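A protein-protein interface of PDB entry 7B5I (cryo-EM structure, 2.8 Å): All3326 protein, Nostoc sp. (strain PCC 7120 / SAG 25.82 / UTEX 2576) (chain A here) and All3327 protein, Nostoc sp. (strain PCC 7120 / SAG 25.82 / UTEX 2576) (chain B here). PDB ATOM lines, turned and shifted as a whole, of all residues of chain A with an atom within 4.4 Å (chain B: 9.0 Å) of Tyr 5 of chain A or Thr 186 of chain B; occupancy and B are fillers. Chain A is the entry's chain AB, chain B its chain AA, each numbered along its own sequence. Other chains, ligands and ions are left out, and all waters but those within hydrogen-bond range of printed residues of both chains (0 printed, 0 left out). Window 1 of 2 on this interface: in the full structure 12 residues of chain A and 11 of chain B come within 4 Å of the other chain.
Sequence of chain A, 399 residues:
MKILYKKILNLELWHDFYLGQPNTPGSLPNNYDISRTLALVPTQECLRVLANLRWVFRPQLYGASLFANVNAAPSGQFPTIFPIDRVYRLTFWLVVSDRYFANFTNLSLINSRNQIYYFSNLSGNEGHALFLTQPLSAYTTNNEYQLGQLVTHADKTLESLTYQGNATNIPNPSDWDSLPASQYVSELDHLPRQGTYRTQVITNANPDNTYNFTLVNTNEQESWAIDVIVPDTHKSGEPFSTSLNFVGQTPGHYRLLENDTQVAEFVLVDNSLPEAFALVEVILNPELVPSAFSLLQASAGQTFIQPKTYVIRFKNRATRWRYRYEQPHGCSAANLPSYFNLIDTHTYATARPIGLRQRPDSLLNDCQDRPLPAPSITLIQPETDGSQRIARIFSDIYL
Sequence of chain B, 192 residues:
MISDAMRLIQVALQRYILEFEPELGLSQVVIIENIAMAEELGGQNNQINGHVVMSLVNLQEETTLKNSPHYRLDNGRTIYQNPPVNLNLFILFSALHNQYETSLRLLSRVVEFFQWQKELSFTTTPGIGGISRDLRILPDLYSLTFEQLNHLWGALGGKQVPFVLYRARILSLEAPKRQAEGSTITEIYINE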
ATOM      1  N   ILE A   3       3.916  10.964  23.020  1.00  0.00           N
ATOM      2  CA  ILE A   3       2.467  10.921  23.175  1.00  0.00           C
ATOM      3  C   ILE A   3       1.952  12.343  23.309  1.00  0.00           C
ATOM      4  O   ILE A   3       2.254  13.024  24.295  1.00  0.00           O
ATOM      5  CB  ILE A   3       2.043  10.082  24.387  1.00  0.00           C
ATOM      6  CG1 ILE A   3       2.729   8.721  24.355  1.00  0.00           C
ATOM      7  CG2 ILE A   3       0.546   9.904  24.397  1.00  0.00           C
ATOM      8  CD1 ILE A   3       2.409   7.864  25.538  1.00  0.00           C
ATOM      9  N   LEU A   4       1.161  12.784  22.337  1.00  0.00           N
ATOM     10  CA  LEU A   4       0.608  14.128  22.324  1.00  0.00           C
ATOM     11  C   LEU A   4      -0.893  14.095  22.578  1.00  0.00           C
ATOM     12  O   LEU A   4      -1.626  13.331  21.939  1.00  0.00           O
ATOM     13  CB  LEU A   4       0.893  14.812  20.989  1.00  0.00           C
ATOM     14  CG  LEU A   4       0.824  16.334  20.965  1.00  0.00           C
ATOM     15  CD1 LEU A   4       1.692  16.912  22.050  1.00  0.00           C
ATOM     16  CD2 LEU A   4       1.250  16.848  19.611  1.00  0.00           C
ATOM     17  N   TYR A   5      -1.351  14.971  23.472  1.00  0.00           N
ATOM     18  CA  TYR A   5      -2.745  15.043  23.881  1.00  0.00           C
ATOM     19  C   TYR A   5      -3.278  16.443  23.623  1.00  0.00           C
ATOM     20  O   TYR A   5      -2.550  17.428  23.766  1.00  0.00           O
ATOM     21  CB  TYR A   5      -2.918  14.703  25.363  1.00  0.00           C
ATOM     22  CG  TYR A   5      -2.781  13.236  25.691  1.00  0.00           C
ATOM     23  CD1 TYR A   5      -3.709  12.315  25.238  1.00  0.00           C
ATOM     24  CD2 TYR A   5      -1.724  12.778  26.463  1.00  0.00           C
ATOM     25  CE1 TYR A   5      -3.585  10.977  25.538  1.00  0.00           C
ATOM     26  CE2 TYR A   5      -1.593  11.447  26.768  1.00  0.00           C
ATOM     27  CZ  TYR A   5      -2.526  10.547  26.304  1.00  0.00           C
ATOM     28  OH  TYR A   5      -2.399   9.212  26.605  1.00  0.00           O
ATOM     29  N   LYS A   6      -4.543  16.532  23.233  1.00  0.00           N
ATOM     30  CA  LYS A   6      -5.170  17.818  22.964  1.00  0.00           C
ATOM     31  C   LYS A   6      -6.619  17.786  23.424  1.00  0.00           C
ATOM     32  O   LYS A   6      -7.306  16.779  23.257  1.00  0.00           O
ATOM     33  CB  LYS A   6      -5.105  18.152  21.471  1.00  0.00           C
ATOM     34  CG  LYS A   6      -3.719  18.518  20.967  1.00  0.00           C
ATOM     35  CD  LYS A   6      -3.196  19.770  21.652  1.00  0.00           C
ATOM     36  CE  LYS A   6      -1.809  20.137  21.148  1.00  0.00           C
ATOM     37  NZ  LYS A   6      -1.282  21.359  21.816  1.00  0.00           N
ATOM     38  N   ALA A  68      -7.886  13.929  23.486  1.00  0.00           N
ATOM     39  CA  ALA A  68      -7.597  12.958  22.447  1.00  0.00           C
ATOM     40  C   ALA A  68      -6.097  12.882  22.195  1.00  0.00           C
ATOM     41  O   ALA A  68      -5.356  13.844  22.408  1.00  0.00           O
ATOM     42  CB  ALA A  68      -8.328  13.312  21.150  1.00  0.00           C
ATOM     43  N   ASN A  69      -5.663  11.718  21.727  1.00  0.00           N
ATOM     44  CA  ASN A  69      -4.262  11.445  21.431  1.00  0.00           C
ATOM     45  C   ASN A  69      -4.055  11.646  19.934  1.00  0.00           C
ATOM     46  O   ASN A  69      -4.620  10.909  19.122  1.00  0.00           O
ATOM     47  CB  ASN A  69      -3.903  10.027  21.868  1.00  0.00           C
ATOM     48  CG  ASN A  69      -2.448   9.684  21.629  1.00  0.00           C
ATOM     49  OD1 ASN A  69      -1.631  10.546  21.303  1.00  0.00           O
ATOM     50  ND2 ASN A  69      -2.114   8.413  21.795  1.00  0.00           N
ATOM     51  N   GLY B  76      -5.575  26.138  31.743  1.00  0.00           N
ATOM     52  CA  GLY B  76      -4.402  25.345  31.440  1.00  0.00           C
ATOM     53  C   GLY B  76      -3.096  25.912  31.941  1.00  0.00           C
ATOM     54  O   GLY B  76      -2.035  25.476  31.486  1.00  0.00           O
ATOM     55  N   ARG B  77      -3.134  26.883  32.848  1.00  0.00           N
ATOM     56  CA  ARG B  77      -1.929  27.446  33.433  1.00  0.00           C
ATOM     57  C   ARG B  77      -2.058  27.461  34.949  1.00  0.00           C
ATOM     58  O   ARG B  77      -3.155  27.361  35.502  1.00  0.00           O
ATOM     59  CB  ARG B  77      -1.656  28.853  32.902  1.00  0.00           C
ATOM     60  CG  ARG B  77      -1.446  28.890  31.405  1.00  0.00           C
ATOM     61  CD  ARG B  77      -0.716  30.142  30.978  1.00  0.00           C
ATOM     62  NE  ARG B  77       0.669  30.142  31.442  1.00  0.00           N
ATOM     63  CZ  ARG B  77       1.144  30.970  32.365  1.00  0.00           C
ATOM     64  NH1 ARG B  77       0.347  31.868  32.926  1.00  0.00           N
ATOM     65  NH2 ARG B  77       2.417  30.900  32.725  1.00  0.00           N
ATOM     66  N   SER B 183       3.096  26.557  33.654  1.00  0.00           N
ATOM     67  CA  SER B 183       2.335  25.823  32.651  1.00  0.00           C
ATOM     68  C   SER B 183       2.213  24.355  33.043  1.00  0.00           C
ATOM     69  O   SER B 183       2.966  23.848  33.875  1.00  0.00           O
ATOM     70  CB  SER B 183       2.974  25.939  31.259  1.00  0.00           C
ATOM     71  OG  SER B 183       4.226  25.283  31.207  1.00  0.00           O
ATOM     72  N   THR B 184       1.246  23.674  32.426  1.00  0.00           N
ATOM     73  CA  THR B 184       0.892  22.304  32.767  1.00  0.00           C
ATOM     74  C   THR B 184       1.491  21.310  31.775  1.00  0.00           C
ATOM     75  O   THR B 184       2.226  21.669  30.853  1.00  0.00           O
ATOM     76  CB  THR B 184      -0.627  22.139  32.835  1.00  0.00           C
ATOM     77  OG1 THR B 184      -1.193  22.389  31.545  1.00  0.00           O
ATOM     78  CG2 THR B 184      -1.230  23.100  33.844  1.00  0.00           C
ATOM     79  N   ILE B 185       1.162  20.036  31.977  1.00  0.00           N
ATOM     80  CA  ILE B 185       1.731  18.932  31.209  1.00  0.00           C
ATOM     81  C   ILE B 185       0.830  18.609  30.027  1.00  0.00           C
ATOM     82  O   ILE B 185      -0.376  18.410  30.192  1.00  0.00           O
ATOM     83  CB  ILE B 185       1.919  17.695  32.099  1.00  0.00           C
ATOM     84  CG1 ILE B 185       3.021  17.941  33.126  1.00  0.00           C
ATOM     85  CG2 ILE B 185       2.233  16.476  31.266  1.00  0.00           C
ATOM     86  CD1 ILE B 185       3.045  16.923  34.237  1.00  0.00           C
ATOM     87  N   THR B 186       1.417  18.527  28.834  1.00  0.00           N
ATOM     88  CA  THR B 186       0.661  18.200  27.630  1.00  0.00           C
ATOM     89  C   THR B 186       1.315  17.140  26.748  1.00  0.00           C
ATOM     90  O   THR B 186       0.626  16.562  25.902  1.00  0.00           O
ATOM     91  CB  THR B 186       0.421  19.466  26.793  1.00  0.00           C
ATOM     92  OG1 THR B 186       0.037  20.538  27.661  1.00  0.00           O
ATOM     93  CG2 THR B 186      -0.707  19.248  25.800  1.00  0.00           C
ATOM     94  N   GLU B 187       2.600  16.846  26.925  1.00  0.00           N
ATOM     95  CA  GLU B 187       3.266  15.833  26.117  1.00  0.00           C
ATOM     96  C   GLU B 187       4.267  15.089  26.985  1.00  0.00           C
ATOM     97  O   GLU B 187       4.891  15.684  27.865  1.00  0.00           O
ATOM     98  CB  GLU B 187       3.978  16.451  24.912  1.00  0.00           C
ATOM     99  CG  GLU B 187       4.587  15.430  23.972  1.00  0.00           C
ATOM    100  CD  GLU B 187       5.230  16.061  22.759  1.00  0.00           C
ATOM    101  OE1 GLU B 187       5.279  17.305  22.687  1.00  0.00           O
ATOM    102  OE2 GLU B 187       5.671  15.308  21.865  1.00  0.00           O
ATOM    103  N   ILE B 188       4.441  13.778  26.756  1.00  0.00           N
ATOM    104  CA  ILE B 188       5.389  12.933  27.517  1.00  0.00           C
ATOM    105  C   ILE B 188       6.229  12.009  26.596  1.00  0.00           C
ATOM    106  O   ILE B 188       5.683  11.420  25.663  1.00  0.00           O
ATOM    107  CB  ILE B 188       4.641  12.052  28.558  1.00  0.00           C
ATOM    108  CG1 ILE B 188       3.832  12.903  29.541  1.00  0.00           C
ATOM    109  CG2 ILE B 188       5.601  11.172  29.347  1.00  0.00           C
ATOM    110  CD1 ILE B 188       3.089  12.094  30.581  1.00  0.00           C
ATOM    111  N   TYR B 189       7.541  11.917  26.813  1.00  0.00           N
ATOM    112  CA  TYR B 189       8.375  11.007  26.041  1.00  0.00           C
ATOM    113  C   TYR B 189       8.856   9.984  27.006  1.00  0.00           C
ATOM    114  O   TYR B 189       9.279  10.333  28.078  1.00  0.00           O
ATOM    115  CB  TYR B 189       9.666  11.612  25.509  1.00  0.00           C
ATOM    116  CG  TYR B 189       9.621  12.729  24.481  1.00  0.00           C
ATOM    117  CD1 TYR B 189       9.555  12.479  23.134  1.00  0.00           C
ATOM    118  CD2 TYR B 189       9.690  14.036  24.895  1.00  0.00           C
ATOM    119  CE1 TYR B 189       9.518  13.498  22.235  1.00  0.00           C
ATOM    120  CE2 TYR B 189       9.649  15.068  24.009  1.00  0.00           C
ATOM    121  CZ  TYR B 189       9.564  14.794  22.675  1.00  0.00           C
ATOM    122  OH  TYR B 189       9.530  15.834  21.791  1.00  0.00           O
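Among the printed residues, merely in contact across the chains: Ile 3 of chain A with Glu 187 of chain B, Leu 4 of chain A with Glu 187 of chain B and Tyr 5 of chain A with Thr 186 of chain B.
O of Leu 4 of chain A sits close to OD1 of Asn 69 of chain A (2.9 Å).
Printed residues of chain B within 4 Å of Ile 3 of chain A: Glu 187 (3.4 Å) and Ile 188 (3.2 Å). Printed residues of chain B within 4 Å of Tyr 5 of chain A: Thr 186. Gly 76 of chain B touches none of the printed residues of chain A. Ser 183 of chain B touches none of the printed residues of chain A. Of the printed residues of chain A, Thr 186 of chain B touches Tyr 5 (3.3 Å). Printed residues of chain A within 4 Å of Glu 187 of chain B: Ile 3 and Leu 4. The nearest residue of chain B that does not touch Tyr 5 of chain A is Glu 187 of chain B (5.4 Å).
Printed residues of chain B that touch a printed residue of chain A: Thr 186, Glu 187 and Ile 188. Of the 6 printed residues of chain A, 3 touch a printed residue of chain B. Hydrophobic or aromatic side chains of chain A within 4 Å of the printed part of chain B: Leu 4. Among the printed residues, 4 pairs touch across the chains.
The backbone carbonyl oxygen (O) of Ile 188 of chain B sits at hydrogen-bond distance from the backbone NH (N) of Ile 3 of chain A, 3.2 Å away.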
